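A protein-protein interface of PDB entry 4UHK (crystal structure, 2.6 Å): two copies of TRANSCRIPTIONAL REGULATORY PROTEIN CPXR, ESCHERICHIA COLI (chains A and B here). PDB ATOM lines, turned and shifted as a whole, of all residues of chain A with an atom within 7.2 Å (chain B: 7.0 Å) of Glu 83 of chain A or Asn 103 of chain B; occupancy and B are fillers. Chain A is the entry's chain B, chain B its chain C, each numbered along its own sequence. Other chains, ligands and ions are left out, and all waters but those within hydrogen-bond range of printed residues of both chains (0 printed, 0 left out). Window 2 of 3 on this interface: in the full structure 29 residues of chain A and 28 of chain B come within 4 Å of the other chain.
The side-chain carboxylate of Glu 106 of chain B is in salt-bridge range of the guanidinium group of Arg 86 of chain A, at 3.3 Å.
The guanidinium group (NH1) of Arg 86 of chain A lies within hydrogen-bond range of the backbone carbonyl oxygen (O) of Gly 81 of chain A, at 2.8 Å. The side-chain amide oxygen (OD1) of Asn 103 of chain B sits at hydrogen-bond distance from the backbone NH (N) of Glu 106 of chain B, at 3.5 Å.
OE2 of Glu 83 of chain A touches CB of Asn 103 of chain B, at 3.4 Å. CG1 of Val 87 of chain A touches NH2 of Arg 105 of chain B, 3.6 Å away. Val 87 of chain A touches Glu 106 of chain B (CG2 to N, 3.5 Å). CB of Leu 90 of chain A touches CB of Ala 109 of chain B (3.99 Å).
Glu 83 of chain A touches one residue of chain B. Of the printed residues of chain A, Asn 103 of chain B touches Glu 83 (3.4 Å). Of the printed residues of chain A, Glu 106 of chain B touches Arg 86 (3.3 Å) and Val 87 (3.5 Å). Printed residues of chain A within 4 Å of Ala 109 of chain B: Leu 90 (3.99 Å). The nearest residue of chain B that does not touch Glu 83 of chain A is Glu 106 of chain B (4.5 Å).
Printed residues of chain A that touch a printed residue of chain B: Glu 83, Arg 86, Val 87 and Leu 90. Hydrophobic or aromatic side chains of chain A that line the printed part of chain B: Val 87 and Leu 90. Of the 11 printed residues of chain B, 4 touch a printed residue of chain A. Printed residues of chain B that touch a printed residue of chain A: Asn 103, Arg 105, Glu 106 and Ala 109. Among the printed residues, 5 pairs touch across the chains. Among the printed residues, Asp or Glu carboxylates within 4 Å of a Lys or Arg side-chain nitrogen of the other chain: Arg 86 of chain A with Glu 106 of chain B.
No position is printed for both chains. Of the 5 pairs that touch across the chains among the printed residues, none has its exchanged pair printed and touching as well.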
ATOM      1  N   ARG A  80      22.304  -3.040 -13.719  1.00  0.00           N
ATOM      2  CA  ARG A  80      21.092  -3.267 -12.932  1.00  0.00           C
ATOM      3  C   ARG A  80      19.935  -2.529 -13.591  1.00  0.00           C
ATOM      4  O   ARG A  80      19.690  -1.359 -13.294  1.00  0.00           O
ATOM      5  CB  ARG A  80      21.319  -2.802 -11.482  1.00  0.00           C
ATOM      6  CG  ARG A  80      22.293  -3.707 -10.695  1.00  0.00           C
ATOM      7  CD  ARG A  80      21.612  -5.023 -10.395  1.00  0.00           C
ATOM      8  NE  ARG A  80      22.495  -6.012  -9.812  1.00  0.00           N
ATOM      9  CZ  ARG A  80      22.583  -6.204  -8.507  1.00  0.00           C
ATOM     10  NH1 ARG A  80      21.883  -5.446  -7.667  1.00  0.00           N
ATOM     11  NH2 ARG A  80      23.364  -7.160  -8.028  1.00  0.00           N
ATOM     12  N   GLY A  81      19.292  -3.189 -14.552  1.00  0.00           N
ATOM     13  CA  GLY A  81      18.277  -2.543 -15.361  1.00  0.00           C
ATOM     14  C   GLY A  81      16.850  -2.988 -15.229  1.00  0.00           C
ATOM     15  O   GLY A  81      16.029  -2.616 -16.076  1.00  0.00           O
ATOM     16  N   SER A  82      16.522  -3.741 -14.170  1.00  0.00           N
ATOM     17  CA  SER A  82      15.136  -4.158 -13.957  1.00  0.00           C
ATOM     18  C   SER A  82      14.267  -2.952 -13.553  1.00  0.00           C
ATOM     19  O   SER A  82      14.801  -1.943 -13.090  1.00  0.00           O
ATOM     20  CB  SER A  82      15.060  -5.240 -12.893  1.00  0.00           C
ATOM     21  OG  SER A  82      15.021  -4.682 -11.592  1.00  0.00           O
ATOM     22  N   GLU A  83      12.940  -3.066 -13.713  1.00  0.00           N
ATOM     23  CA  GLU A  83      11.972  -2.032 -13.328  1.00  0.00           C
ATOM     24  C   GLU A  83      12.153  -1.664 -11.833  1.00  0.00           C
ATOM     25  O   GLU A  83      12.149  -0.480 -11.500  1.00  0.00           O
ATOM     26  CB  GLU A  83      10.539  -2.509 -13.623  1.00  0.00           C
ATOM     27  CG  GLU A  83      10.246  -2.607 -15.121  1.00  0.00           C
ATOM     28  CD  GLU A  83       9.038  -3.408 -15.585  1.00  0.00           C
ATOM     29  OE1 GLU A  83       8.743  -4.464 -14.979  1.00  0.00           O
ATOM     30  OE2 GLU A  83       8.438  -3.021 -16.613  1.00  0.00           O
ATOM     31  N   LEU A  84      12.423  -2.675 -10.966  1.00  0.00           N
ATOM     32  CA  LEU A  84      12.683  -2.505  -9.538  1.00  0.00           C
ATOM     33  C   LEU A  84      13.944  -1.665  -9.317  1.00  0.00           C
ATOM     34  O   LEU A  84      13.884  -0.675  -8.584  1.00  0.00           O
ATOM     35  CB  LEU A  84      12.802  -3.867  -8.846  1.00  0.00           C
ATOM     36  CG  LEU A  84      11.612  -4.891  -8.962  1.00  0.00           C
ATOM     37  CD1 LEU A  84      11.549  -5.771  -7.743  1.00  0.00           C
ATOM     38  CD2 LEU A  84      10.212  -4.222  -9.115  1.00  0.00           C
ATOM     39  N   ASP A  85      15.061  -2.035  -9.987  1.00  0.00           N
ATOM     40  CA  ASP A  85      16.340  -1.327  -9.948  1.00  0.00           C
ATOM     41  C   ASP A  85      16.162   0.157 -10.314  1.00  0.00           C
ATOM     42  O   ASP A  85      16.631   1.030  -9.578  1.00  0.00           O
ATOM     43  CB  ASP A  85      17.346  -1.988 -10.910  1.00  0.00           C
ATOM     44  CG  ASP A  85      17.744  -3.415 -10.574  1.00  0.00           C
ATOM     45  OD1 ASP A  85      17.880  -3.729  -9.368  1.00  0.00           O
ATOM     46  OD2 ASP A  85      17.946  -4.212 -11.516  1.00  0.00           O
ATOM     47  N   ARG A  86      15.449   0.430 -11.434  1.00  0.00           N
ATOM     48  CA  ARG A  86      15.170   1.772 -11.957  1.00  0.00           C
ATOM     49  C   ARG A  86      14.346   2.594 -10.958  1.00  0.00           C
ATOM     50  O   ARG A  86      14.789   3.683 -10.581  1.00  0.00           O
ATOM     51  CB  ARG A  86      14.470   1.700 -13.324  1.00  0.00           C
ATOM     52  CG  ARG A  86      15.283   0.955 -14.381  1.00  0.00           C
ATOM     53  CD  ARG A  86      14.795   1.224 -15.784  1.00  0.00           C
ATOM     54  NE  ARG A  86      13.734   0.310 -16.194  1.00  0.00           N
ATOM     55  CZ  ARG A  86      13.854  -0.596 -17.149  1.00  0.00           C
ATOM     56  NH1 ARG A  86      14.979  -0.706 -17.831  1.00  0.00           N
ATOM     57  NH2 ARG A  86      12.839  -1.388 -17.444  1.00  0.00           N
ATOM     58  N   VAL A  87      13.195   2.057 -10.481  1.00  0.00           N
ATOM     59  CA  VAL A  87      12.315   2.727  -9.505  1.00  0.00           C
ATOM     60  C   VAL A  87      13.097   3.031  -8.201  1.00  0.00           C
ATOM     61  O   VAL A  87      12.952   4.126  -7.655  1.00  0.00           O
ATOM     62  CB  VAL A  87      11.012   1.908  -9.259  1.00  0.00           C
ATOM     63  CG1 VAL A  87      10.216   2.408  -8.052  1.00  0.00           C
ATOM     64  CG2 VAL A  87      10.139   1.905 -10.507  1.00  0.00           C
ATOM     65  N   LEU A  88      13.951   2.099  -7.747  1.00  0.00           N
ATOM     66  CA  LEU A  88      14.758   2.268  -6.539  1.00  0.00           C
ATOM     67  C   LEU A  88      15.739   3.441  -6.681  1.00  0.00           C
ATOM     68  O   LEU A  88      15.800   4.295  -5.798  1.00  0.00           O
ATOM     69  CB  LEU A  88      15.509   0.955  -6.201  1.00  0.00           C
ATOM     70  CG  LEU A  88      16.336   0.928  -4.888  1.00  0.00           C
ATOM     71  CD1 LEU A  88      15.449   0.985  -3.666  1.00  0.00           C
ATOM     72  CD2 LEU A  88      17.252  -0.268  -4.844  1.00  0.00           C
ATOM     73  N   GLY A  89      16.464   3.482  -7.794  1.00  0.00           N
ATOM     74  CA  GLY A  89      17.436   4.536  -8.088  1.00  0.00           C
ATOM     75  C   GLY A  89      16.806   5.915  -8.092  1.00  0.00           C
ATOM     76  O   GLY A  89      17.313   6.845  -7.450  1.00  0.00           O
ATOM     77  N   LEU A  90      15.643   6.016  -8.754  1.00  0.00           N
ATOM     78  CA  LEU A  90      14.879   7.245  -8.913  1.00  0.00           C
ATOM     79  C   LEU A  90      14.307   7.724  -7.597  1.00  0.00           C
ATOM     80  O   LEU A  90      14.418   8.915  -7.288  1.00  0.00           O
ATOM     81  CB  LEU A  90      13.770   7.047  -9.971  1.00  0.00           C
ATOM     82  CG  LEU A  90      14.295   6.897 -11.428  1.00  0.00           C
ATOM     83  CD1 LEU A  90      13.330   6.142 -12.289  1.00  0.00           C
ATOM     84  CD2 LEU A  90      14.623   8.219 -12.024  1.00  0.00           C
ATOM     85  N   LEU B  98       9.892   7.991 -21.859  1.00  0.00           N
ATOM     86  CA  LEU B  98       9.519   6.655 -21.404  1.00  0.00           C
ATOM     87  C   LEU B  98       8.677   5.952 -22.464  1.00  0.00           C
ATOM     88  O   LEU B  98       7.517   6.312 -22.668  1.00  0.00           O
ATOM     89  CB  LEU B  98       8.780   6.716 -20.036  1.00  0.00           C
ATOM     90  CG  LEU B  98       8.450   5.392 -19.327  1.00  0.00           C
ATOM     91  CD1 LEU B  98       9.698   4.669 -18.852  1.00  0.00           C
ATOM     92  CD2 LEU B  98       7.530   5.632 -18.141  1.00  0.00           C
ATOM     93  N   PRO B  99       9.248   4.931 -23.147  1.00  0.00           N
ATOM     94  CA  PRO B  99       8.474   4.221 -24.178  1.00  0.00           C
ATOM     95  C   PRO B  99       7.308   3.387 -23.618  1.00  0.00           C
ATOM     96  O   PRO B  99       7.318   2.982 -22.448  1.00  0.00           O
ATOM     97  CB  PRO B  99       9.521   3.303 -24.836  1.00  0.00           C
ATOM     98  CG  PRO B  99      10.861   3.873 -24.436  1.00  0.00           C
ATOM     99  CD  PRO B  99      10.632   4.413 -23.069  1.00  0.00           C
ATOM    100  N   PRO B 101       5.117  -0.270 -24.177  1.00  0.00           N
ATOM    101  CA  PRO B 101       4.476  -0.373 -22.850  1.00  0.00           C
ATOM    102  C   PRO B 101       5.450   0.023 -21.737  1.00  0.00           C
ATOM    103  O   PRO B 101       6.680  -0.120 -21.874  1.00  0.00           O
ATOM    104  CB  PRO B 101       4.055  -1.843 -22.779  1.00  0.00           C
ATOM    105  CG  PRO B 101       5.066  -2.564 -23.618  1.00  0.00           C
ATOM    106  CD  PRO B 101       5.402  -1.608 -24.741  1.00  0.00           C
ATOM    107  N   PHE B 102       4.887   0.589 -20.669  1.00  0.00           N
ATOM    108  CA  PHE B 102       5.638   1.053 -19.514  1.00  0.00           C
ATOM    109  C   PHE B 102       5.077   0.427 -18.223  1.00  0.00           C
ATOM    110  O   PHE B 102       3.955  -0.111 -18.203  1.00  0.00           O
ATOM    111  CB  PHE B 102       5.599   2.602 -19.449  1.00  0.00           C
ATOM    112  CG  PHE B 102       4.230   3.203 -19.220  1.00  0.00           C
ATOM    113  CD1 PHE B 102       3.753   3.426 -17.930  1.00  0.00           C
ATOM    114  CD2 PHE B 102       3.407   3.528 -20.290  1.00  0.00           C
ATOM    115  CE1 PHE B 102       2.468   3.945 -17.719  1.00  0.00           C
ATOM    116  CE2 PHE B 102       2.120   4.044 -20.077  1.00  0.00           C
ATOM    117  CZ  PHE B 102       1.667   4.266 -18.796  1.00  0.00           C
ATOM    118  N   ASN B 103       5.867   0.522 -17.143  1.00  0.00           N
ATOM    119  CA  ASN B 103       5.474   0.106 -15.798  1.00  0.00           C
ATOM    120  C   ASN B 103       5.038   1.370 -15.059  1.00  0.00           C
ATOM    121  O   ASN B 103       5.765   2.368 -15.058  1.00  0.00           O
ATOM    122  CB  ASN B 103       6.611  -0.646 -15.074  1.00  0.00           C
ATOM    123  CG  ASN B 103       6.404  -0.908 -13.589  1.00  0.00           C
ATOM    124  OD1 ASN B 103       7.272  -0.604 -12.775  1.00  0.00           O
ATOM    125  ND2 ASN B 103       5.288  -1.529 -13.192  1.00  0.00           N
ATOM    126  N   ASP B 104       3.826   1.336 -14.485  1.00  0.00           N
ATOM    127  CA  ASP B 104       3.195   2.442 -13.764  1.00  0.00           C
ATOM    128  C   ASP B 104       4.070   2.975 -12.634  1.00  0.00           C
ATOM    129  O   ASP B 104       4.117   4.189 -12.419  1.00  0.00           O
ATOM    130  CB  ASP B 104       1.830   2.013 -13.210  1.00  0.00           C
ATOM    131  CG  ASP B 104       0.728   1.836 -14.251  1.00  0.00           C
ATOM    132  OD1 ASP B 104       0.926   2.265 -15.418  1.00  0.00           O
ATOM    133  OD2 ASP B 104      -0.349   1.302 -13.889  1.00  0.00           O
ATOM    134  N   ARG B 105       4.785   2.075 -11.941  1.00  0.00           N
ATOM    135  CA  ARG B 105       5.680   2.421 -10.835  1.00  0.00           C
ATOM    136  C   ARG B 105       6.839   3.245 -11.342  1.00  0.00           C
ATOM    137  O   ARG B 105       7.190   4.229 -10.690  1.00  0.00           O
ATOM    138  CB  ARG B 105       6.187   1.156 -10.129  1.00  0.00           C
ATOM    139  CG  ARG B 105       5.103   0.395  -9.408  1.00  0.00           C
ATOM    140  CD  ARG B 105       5.101   0.828  -7.966  1.00  0.00           C
ATOM    141  NE  ARG B 105       6.449   0.800  -7.384  1.00  0.00           N
ATOM    142  CZ  ARG B 105       6.710   1.035  -6.104  1.00  0.00           C
ATOM    143  NH1 ARG B 105       5.725   1.313  -5.258  1.00  0.00           N
ATOM    144  NH2 ARG B 105       7.960   0.984  -5.655  1.00  0.00           N
ATOM    145  N   GLU B 106       7.412   2.871 -12.512  1.00  0.00           N
ATOM    146  CA  GLU B 106       8.509   3.591 -13.132  1.00  0.00           C
ATOM    147  C   GLU B 106       8.047   4.958 -13.602  1.00  0.00           C
ATOM    148  O   GLU B 106       8.778   5.931 -13.407  1.00  0.00           O
ATOM    149  CB  GLU B 106       9.129   2.795 -14.278  1.00  0.00           C
ATOM    150  CG  GLU B 106      10.385   3.482 -14.805  1.00  0.00           C
ATOM    151  CD  GLU B 106      11.156   2.804 -15.913  1.00  0.00           C
ATOM    152  OE1 GLU B 106      10.738   1.719 -16.382  1.00  0.00           O
ATOM    153  OE2 GLU B 106      12.208   3.361 -16.295  1.00  0.00           O
ATOM    154  N   LEU B 107       6.833   5.052 -14.196  1.00  0.00           N
ATOM    155  CA  LEU B 107       6.280   6.334 -14.649  1.00  0.00           C
ATOM    156  C   LEU B 107       6.171   7.321 -13.480  1.00  0.00           C
ATOM    157  O   LEU B 107       6.697   8.429 -13.576  1.00  0.00           O
ATOM    158  CB  LEU B 107       4.914   6.160 -15.343  1.00  0.00           C
ATOM    159  CG  LEU B 107       4.151   7.453 -15.661  1.00  0.00           C
ATOM    160  CD1 LEU B 107       4.869   8.312 -16.725  1.00  0.00           C
ATOM    161  CD2 LEU B 107       2.749   7.153 -16.077  1.00  0.00           C
ATOM    162  N   VAL B 108       5.525   6.902 -12.382  1.00  0.00           N
ATOM    163  CA  VAL B 108       5.339   7.700 -11.175  1.00  0.00           C
ATOM    164  C   VAL B 108       6.727   8.128 -10.604  1.00  0.00           C
ATOM    165  O   VAL B 108       6.918   9.313 -10.306  1.00  0.00           O
ATOM    166  CB  VAL B 108       4.462   6.943 -10.134  1.00  0.00           C
ATOM    167  CG1 VAL B 108       4.386   7.706  -8.821  1.00  0.00           C
ATOM    168  CG2 VAL B 108       3.053   6.724 -10.670  1.00  0.00           C
ATOM    169  N   ALA B 109       7.700   7.181 -10.527  1.00  0.00           N
ATOM    170  CA  ALA B 109       9.059   7.436 -10.027  1.00  0.00           C
ATOM    171  C   ALA B 109       9.753   8.513 -10.852  1.00  0.00           C
ATOM    172  O   ALA B 109      10.364   9.399 -10.266  1.00  0.00           O
ATOM    173  CB  ALA B 109       9.879   6.149 -10.027  1.00  0.00           C
